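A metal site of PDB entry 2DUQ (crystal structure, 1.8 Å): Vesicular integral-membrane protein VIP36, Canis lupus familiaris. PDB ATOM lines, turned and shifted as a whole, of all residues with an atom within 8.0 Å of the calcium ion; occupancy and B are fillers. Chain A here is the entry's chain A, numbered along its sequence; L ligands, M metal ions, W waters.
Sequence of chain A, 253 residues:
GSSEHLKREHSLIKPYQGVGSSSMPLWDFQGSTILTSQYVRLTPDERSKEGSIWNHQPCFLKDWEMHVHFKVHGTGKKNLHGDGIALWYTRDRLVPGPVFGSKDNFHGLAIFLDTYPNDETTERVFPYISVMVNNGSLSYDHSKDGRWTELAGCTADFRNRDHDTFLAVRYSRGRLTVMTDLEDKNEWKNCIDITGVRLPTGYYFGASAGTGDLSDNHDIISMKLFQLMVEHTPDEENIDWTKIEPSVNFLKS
Of the 21 residues printed, 4 come within 4 Å of the calcium ion. The nearest printed residue that does not touch the calcium ion is His 142 (4.4 Å).
The backbone NH of Asp 119 lies within hydrogen-bond range of the side-chain carboxylate of Asp 145 (3.0 Å). OH of Tyr 140 lies close to OD1 of Asp 114, at 3.5 Å. The side-chain amide nitrogen (ND2) of Asn 118 is in hydrogen-bond range of a ring nitrogen (NE2) of His 142, at 3.4 Å. The backbone NH (N) of Tyr 128 sits at hydrogen-bond distance from the backbone carbonyl oxygen (O) of Asp 114 (2.9 Å).
Water W2 bridges OH of Tyr 140 (2.8 Å) and ND1 of His 142 (2.9 Å).
The side-chain amide nitrogen (ND2) of Asn 118 lies within hydrogen-bond range of an oxygen (O4) of the ligand (2.9 Å). A ring nitrogen (NE2) of His 142 is in hydrogen-bond range of an oxygen (O3) of the ligand. An oxygen (O4) of the ligand lies within hydrogen-bond range of the side-chain carboxylate of Asp 83 (2.6 Å).
O of Tyr 116 binds the calcium ion. The calcium ion is bound by OD2 of Asp 145 (2.4 Å). The calcium ion is bound by OD1 of Asn 118, at 2.4 Å. Water W1 binds the calcium ion (2.4 Å). OD2 of Asp 114 is bound to the calcium ion. The calcium ion is bound by water W2 (2.5 Å). The calcium ion is bound by OD1 of Asp 114 (2.6 Å).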
ATOM      1  N   HIS A  81       4.974  16.793   7.708  1.00  0.00           N
ATOM      2  CA  HIS A  81       3.604  16.458   7.309  1.00  0.00           C
ATOM      3  C   HIS A  81       3.394  14.947   7.439  1.00  0.00           C
ATOM      4  O   HIS A  81       4.360  14.175   7.461  1.00  0.00           O
ATOM      5  CB  HIS A  81       3.304  16.932   5.894  1.00  0.00           C
ATOM      6  CG  HIS A  81       4.288  16.445   4.879  1.00  0.00           C
ATOM      7  ND1 HIS A  81       5.380  17.181   4.493  1.00  0.00           N
ATOM      8  CD2 HIS A  81       4.366  15.278   4.201  1.00  0.00           C
ATOM      9  CE1 HIS A  81       6.080  16.507   3.609  1.00  0.00           C
ATOM     10  NE2 HIS A  81       5.487  15.339   3.411  1.00  0.00           N
ATOM     11  N   GLY A  82       2.142  14.526   7.574  1.00  0.00           N
ATOM     12  CA  GLY A  82       1.815  13.105   7.669  1.00  0.00           C
ATOM     13  C   GLY A  82       0.308  12.911   7.864  1.00  0.00           C
ATOM     14  O   GLY A  82      -0.401  13.885   8.049  1.00  0.00           O
ATOM     15  N   ASP A  83      -0.178  11.684   7.849  1.00  0.00           N
ATOM     16  CA  ASP A  83       0.647  10.477   7.666  1.00  0.00           C
ATOM     17  C   ASP A  83       0.388   9.805   6.334  1.00  0.00           C
ATOM     18  O   ASP A  83       1.234   9.002   5.876  1.00  0.00           O
ATOM     19  CB  ASP A  83       0.385   9.507   8.811  1.00  0.00           C
ATOM     20  CG  ASP A  83       1.245   9.793  10.000  1.00  0.00           C
ATOM     21  OD1 ASP A  83       0.745  10.474  10.922  1.00  0.00           O
ATOM     22  OD2 ASP A  83       2.427   9.411   9.975  1.00  0.00           O
ATOM     23  N   GLY A  84      -0.792  10.060   5.759  1.00  0.00           N
ATOM     24  CA  GLY A  84      -1.136   9.550   4.447  1.00  0.00           C
ATOM     25  C   GLY A  84      -2.531   8.963   4.381  1.00  0.00           C
ATOM     26  O   GLY A  84      -3.310   9.063   5.339  1.00  0.00           O
ATOM     27  N   PHE A 100      -3.267   4.128   8.804  1.00  0.00           N
ATOM     28  CA  PHE A 100      -3.783   5.331   8.137  1.00  0.00           C
ATOM     29  C   PHE A 100      -5.219   5.589   8.489  1.00  0.00           C
ATOM     30  O   PHE A 100      -6.061   5.784   7.613  1.00  0.00           O
ATOM     31  CB  PHE A 100      -3.537   5.263   6.617  1.00  0.00           C
ATOM     32  CG  PHE A 100      -2.092   5.061   6.269  1.00  0.00           C
ATOM     33  CD1 PHE A 100      -1.220   6.127   6.223  1.00  0.00           C
ATOM     34  CD2 PHE A 100      -1.604   3.778   6.026  1.00  0.00           C
ATOM     35  CE1 PHE A 100       0.136   5.933   5.933  1.00  0.00           C
ATOM     36  CE2 PHE A 100      -0.268   3.585   5.725  1.00  0.00           C
ATOM     37  CZ  PHE A 100       0.612   4.658   5.694  1.00  0.00           C
ATOM     38  N   LEU A 113      -0.780   5.161   0.673  1.00  0.00           N
ATOM     39  CA  LEU A 113      -0.169   6.355   0.122  1.00  0.00           C
ATOM     40  C   LEU A 113       0.482   7.020   1.333  1.00  0.00           C
ATOM     41  O   LEU A 113      -0.099   7.890   1.978  1.00  0.00           O
ATOM     42  CB  LEU A 113      -1.223   7.264  -0.532  1.00  0.00           C
ATOM     43  CG  LEU A 113      -1.703   6.862  -1.927  1.00  0.00           C
ATOM     44  CD1 LEU A 113      -2.645   5.694  -1.797  1.00  0.00           C
ATOM     45  CD2 LEU A 113      -2.470   8.010  -2.534  1.00  0.00           C
ATOM     46  N   ASP A 114       1.711   6.609   1.614  1.00  0.00           N
ATOM     47  CA  ASP A 114       2.408   6.982   2.843  1.00  0.00           C
ATOM     48  C   ASP A 114       3.262   8.230   2.617  1.00  0.00           C
ATOM     49  O   ASP A 114       4.147   8.218   1.768  1.00  0.00           O
ATOM     50  CB  ASP A 114       3.296   5.786   3.251  1.00  0.00           C
ATOM     51  CG  ASP A 114       3.884   5.949   4.635  1.00  0.00           C
ATOM     52  OD1 ASP A 114       4.419   4.936   5.148  1.00  0.00           O
ATOM     53  OD2 ASP A 114       3.805   7.045   5.247  1.00  0.00           O
ATOM     54  N   THR A 115       3.032   9.281   3.394  1.00  0.00           N
ATOM     55  CA  THR A 115       3.730  10.558   3.147  1.00  0.00           C
ATOM     56  C   THR A 115       4.800  10.899   4.176  1.00  0.00           C
ATOM     57  O   THR A 115       5.462  11.932   4.047  1.00  0.00           O
ATOM     58  CB  THR A 115       2.754  11.742   3.130  1.00  0.00           C
ATOM     59  OG1 THR A 115       2.169  11.874   4.435  1.00  0.00           O
ATOM     60  CG2 THR A 115       1.659  11.557   2.041  1.00  0.00           C
ATOM     61  N   TYR A 116       4.953  10.064   5.200  1.00  0.00           N
ATOM     62  CA  TYR A 116       5.945  10.324   6.246  1.00  0.00           C
ATOM     63  C   TYR A 116       6.836   9.094   6.484  1.00  0.00           C
ATOM     64  O   TYR A 116       6.325   8.038   6.791  1.00  0.00           O
ATOM     65  CB  TYR A 116       5.243  10.743   7.552  1.00  0.00           C
ATOM     66  CG  TYR A 116       6.219  11.010   8.645  1.00  0.00           C
ATOM     67  CD1 TYR A 116       7.172  12.021   8.518  1.00  0.00           C
ATOM     68  CD2 TYR A 116       6.227  10.225   9.801  1.00  0.00           C
ATOM     69  CE1 TYR A 116       8.112  12.259   9.510  1.00  0.00           C
ATOM     70  CE2 TYR A 116       7.177  10.457  10.812  1.00  0.00           C
ATOM     71  CZ  TYR A 116       8.100  11.474  10.655  1.00  0.00           C
ATOM     72  OH  TYR A 116       9.031  11.707  11.654  1.00  0.00           O
ATOM     73  N   PRO A 117       8.182   9.254   6.326  1.00  0.00           N
ATOM     74  CA  PRO A 117       9.069   8.122   6.621  1.00  0.00           C
ATOM     75  C   PRO A 117       9.259   7.912   8.114  1.00  0.00           C
ATOM     76  O   PRO A 117      10.127   8.556   8.731  1.00  0.00           O
ATOM     77  CB  PRO A 117      10.414   8.533   5.974  1.00  0.00           C
ATOM     78  CG  PRO A 117      10.405  10.048   5.987  1.00  0.00           C
ATOM     79  CD  PRO A 117       8.929  10.445   5.852  1.00  0.00           C
ATOM     80  N   ASN A 118       8.473   7.023   8.696  1.00  0.00           N
ATOM     81  CA  ASN A 118       8.652   6.648  10.101  1.00  0.00           C
ATOM     82  C   ASN A 118       9.955   5.885  10.329  1.00  0.00           C
ATOM     83  O   ASN A 118      10.509   5.903  11.424  1.00  0.00           O
ATOM     84  CB  ASN A 118       7.479   5.804  10.580  1.00  0.00           C
ATOM     85  CG  ASN A 118       6.186   6.585  10.637  1.00  0.00           C
ATOM     86  OD1 ASN A 118       5.479   6.682   9.628  1.00  0.00           O
ATOM     87  ND2 ASN A 118       5.863   7.126  11.804  1.00  0.00           N
ATOM     88  N   ASP A 119      10.414   5.218   9.281  1.00  0.00           N
ATOM     89  CA  ASP A 119      11.549   4.314   9.408  1.00  0.00           C
ATOM     90  C   ASP A 119      12.797   5.163   9.296  1.00  0.00           C
ATOM     91  O   ASP A 119      13.086   5.694   8.233  1.00  0.00           O
ATOM     92  CB  ASP A 119      11.513   3.282   8.284  1.00  0.00           C
ATOM     93  CG  ASP A 119      12.577   2.193   8.457  1.00  0.00           C
ATOM     94  OD1 ASP A 119      13.498   2.362   9.272  1.00  0.00           O
ATOM     95  OD2 ASP A 119      12.488   1.167   7.755  1.00  0.00           O
ATOM     96  N   PHE A 126      10.127   9.288  -0.255  1.00  0.00           N
ATOM     97  CA  PHE A 126       8.699   9.528   0.044  1.00  0.00           C
ATOM     98  C   PHE A 126       8.095  10.711  -0.721  1.00  0.00           C
ATOM     99  O   PHE A 126       8.826  11.604  -1.170  1.00  0.00           O
ATOM    100  CB  PHE A 126       8.505   9.697   1.568  1.00  0.00           C
ATOM    101  CG  PHE A 126       8.463   8.386   2.301  1.00  0.00           C
ATOM    102  CD1 PHE A 126       9.634   7.632   2.488  1.00  0.00           C
ATOM    103  CD2 PHE A 126       7.254   7.881   2.784  1.00  0.00           C
ATOM    104  CE1 PHE A 126       9.604   6.411   3.130  1.00  0.00           C
ATOM    105  CE2 PHE A 126       7.203   6.648   3.443  1.00  0.00           C
ATOM    106  CZ  PHE A 126       8.365   5.901   3.610  1.00  0.00           C
ATOM    107  N   TYR A 128       5.514   7.319  -0.662  1.00  0.00           N
ATOM    108  CA  TYR A 128       5.740   5.999  -1.178  1.00  0.00           C
ATOM    109  C   TYR A 128       4.399   5.260  -1.182  1.00  0.00           C
ATOM    110  O   TYR A 128       3.703   5.211  -0.150  1.00  0.00           O
ATOM    111  CB  TYR A 128       6.776   5.272  -0.296  1.00  0.00           C
ATOM    112  CG  TYR A 128       7.240   4.002  -0.941  1.00  0.00           C
ATOM    113  CD1 TYR A 128       8.178   4.025  -1.983  1.00  0.00           C
ATOM    114  CD2 TYR A 128       6.734   2.768  -0.540  1.00  0.00           C
ATOM    115  CE1 TYR A 128       8.592   2.838  -2.591  1.00  0.00           C
ATOM    116  CE2 TYR A 128       7.160   1.574  -1.151  1.00  0.00           C
ATOM    117  CZ  TYR A 128       8.089   1.623  -2.158  1.00  0.00           C
ATOM    118  OH  TYR A 128       8.498   0.458  -2.766  1.00  0.00           O
ATOM    119  N   TYR A 140       0.429  -4.254  10.355  1.00  0.00           N
ATOM    120  CA  TYR A 140       1.188  -3.257   9.624  1.00  0.00           C
ATOM    121  C   TYR A 140       2.120  -2.560  10.620  1.00  0.00           C
ATOM    122  O   TYR A 140       1.684  -1.969  11.600  1.00  0.00           O
ATOM    123  CB  TYR A 140       0.215  -2.253   9.004  1.00  0.00           C
ATOM    124  CG  TYR A 140       0.895  -1.058   8.365  1.00  0.00           C
ATOM    125  CD1 TYR A 140       1.457  -1.147   7.102  1.00  0.00           C
ATOM    126  CD2 TYR A 140       0.925   0.184   9.035  1.00  0.00           C
ATOM    127  CE1 TYR A 140       2.070  -0.037   6.490  1.00  0.00           C
ATOM    128  CE2 TYR A 140       1.518   1.282   8.438  1.00  0.00           C
ATOM    129  CZ  TYR A 140       2.084   1.171   7.176  1.00  0.00           C
ATOM    130  OH  TYR A 140       2.699   2.255   6.596  1.00  0.00           O
ATOM    131  N   ASP A 141       3.429  -2.655  10.410  1.00  0.00           N
ATOM    132  CA  ASP A 141       4.360  -2.007  11.317  1.00  0.00           C
ATOM    133  C   ASP A 141       4.514  -0.543  10.921  1.00  0.00           C
ATOM    134  O   ASP A 141       5.354  -0.185  10.101  1.00  0.00           O
ATOM    135  CB  ASP A 141       5.726  -2.721  11.325  1.00  0.00           C
ATOM    136  CG  ASP A 141       6.657  -2.146  12.363  1.00  0.00           C
ATOM    137  OD1 ASP A 141       7.681  -2.777  12.672  1.00  0.00           O
ATOM    138  OD2 ASP A 141       6.350  -1.063  12.934  1.00  0.00           O
ATOM    139  N   HIS A 142       3.650   0.292  11.492  1.00  0.00           N
ATOM    140  CA  HIS A 142       3.611   1.712  11.163  1.00  0.00           C
ATOM    141  C   HIS A 142       4.968   2.404  11.398  1.00  0.00           C
ATOM    142  O   HIS A 142       5.405   3.208  10.574  1.00  0.00           O
ATOM    143  CB  HIS A 142       2.474   2.376  11.939  1.00  0.00           C
ATOM    144  CG  HIS A 142       2.456   3.866  11.786  1.00  0.00           C
ATOM    145  ND1 HIS A 142       2.079   4.494  10.630  1.00  0.00           N
ATOM    146  CD2 HIS A 142       2.814   4.849  12.646  1.00  0.00           C
ATOM    147  CE1 HIS A 142       2.188   5.805  10.781  1.00  0.00           C
ATOM    148  NE2 HIS A 142       2.637   6.036  11.996  1.00  0.00           N
ATOM    149  N   SER A 143       5.638   2.029  12.498  1.00  0.00           N
ATOM    150  CA  SER A 143       6.938   2.645  12.841  1.00  0.00           C
ATOM    151  C   SER A 143       8.009   2.406  11.799  1.00  0.00           C
ATOM    152  O   SER A 143       9.019   3.134  11.750  1.00  0.00           O
ATOM    153  CB  SER A 143       7.417   2.167  14.211  1.00  0.00           C
ATOM    154  OG  SER A 143       7.898   0.831  14.152  1.00  0.00           O
ATOM    155  N   LYS A 144       7.800   1.379  10.963  1.00  0.00           N
ATOM    156  CA  LYS A 144       8.716   0.991   9.917  1.00  0.00           C
ATOM    157  C   LYS A 144       8.092   1.122   8.516  1.00  0.00           C
ATOM    158  O   LYS A 144       8.562   0.502   7.567  1.00  0.00           O
ATOM    159  CB  LYS A 144       9.232  -0.440  10.201  1.00  0.00           C
ATOM    160  CG  LYS A 144      10.166  -0.545  11.418  1.00  0.00           C
ATOM    161  CD  LYS A 144      11.452   0.250  11.127  1.00  0.00           C
ATOM    162  CE  LYS A 144      12.701  -0.424  11.617  1.00  0.00           C
ATOM    163  NZ  LYS A 144      13.900   0.114  10.862  1.00  0.00           N
ATOM    164  N   ASP A 145       7.036   1.936   8.380  1.00  0.00           N
ATOM    165  CA  ASP A 145       6.361   2.170   7.093  1.00  0.00           C
ATOM    166  C   ASP A 145       5.969   0.862   6.378  1.00  0.00           C
ATOM    167  O   ASP A 145       6.032   0.792   5.154  1.00  0.00           O
ATOM    168  CB  ASP A 145       7.211   3.026   6.131  1.00  0.00           C
ATOM    169  CG  ASP A 145       7.739   4.289   6.793  1.00  0.00           C
ATOM    170  OD1 ASP A 145       8.977   4.533   6.740  1.00  0.00           O
ATOM    171  OD2 ASP A 145       6.916   5.015   7.380  1.00  0.00           O
ATOM    172  N   GLY A 146       5.640  -0.157   7.158  1.00  0.00           N
ATOM    173  CA  GLY A 146       5.110  -1.421   6.617  1.00  0.00           C
ATOM    174  C   GLY A 146       6.152  -2.264   5.911  1.00  0.00           C
ATOM    175  O   GLY A 146       5.829  -3.130   5.084  1.00  0.00           O
HETATM  176  C1  LIG L   1       3.589  10.683  16.011  1.00  0.00           C
HETATM  177  C2  LIG L   1       2.930   9.311  15.949  1.00  0.00           C
HETATM  178  C3  LIG L   1       3.363   8.577  14.671  1.00  0.00           C
HETATM  179  C4  LIG L   1       3.103   9.443  13.429  1.00  0.00           C
HETATM  180  C5  LIG L   1       3.829  10.777  13.606  1.00  0.00           C
HETATM  181  C6  LIG L   1       3.637  11.740  12.410  1.00  0.00           C
HETATM  182  O1  LIG L   1       4.987  10.559  16.296  1.00  0.00           O
HETATM  183  O2  LIG L   1       1.513   9.445  16.045  1.00  0.00           O
HETATM  184  O3  LIG L   1       2.703   7.336  14.571  1.00  0.00           O
HETATM  185  O4  LIG L   1       3.539   8.791  12.266  1.00  0.00           O
HETATM  186  O5  LIG L   1       3.365  11.397  14.798  1.00  0.00           O
HETATM  187  O6  LIG L   1       2.310  12.215  12.379  1.00  0.00           O
HETATM  188 CA    CA M   1       4.906   6.274   7.324  1.00  0.00          CA
HETATM  189  O   HOH W   1       3.112   7.814   7.842  1.00  0.00           O
HETATM  190  O   HOH W   2       3.602   4.330   8.181  1.00  0.00           O
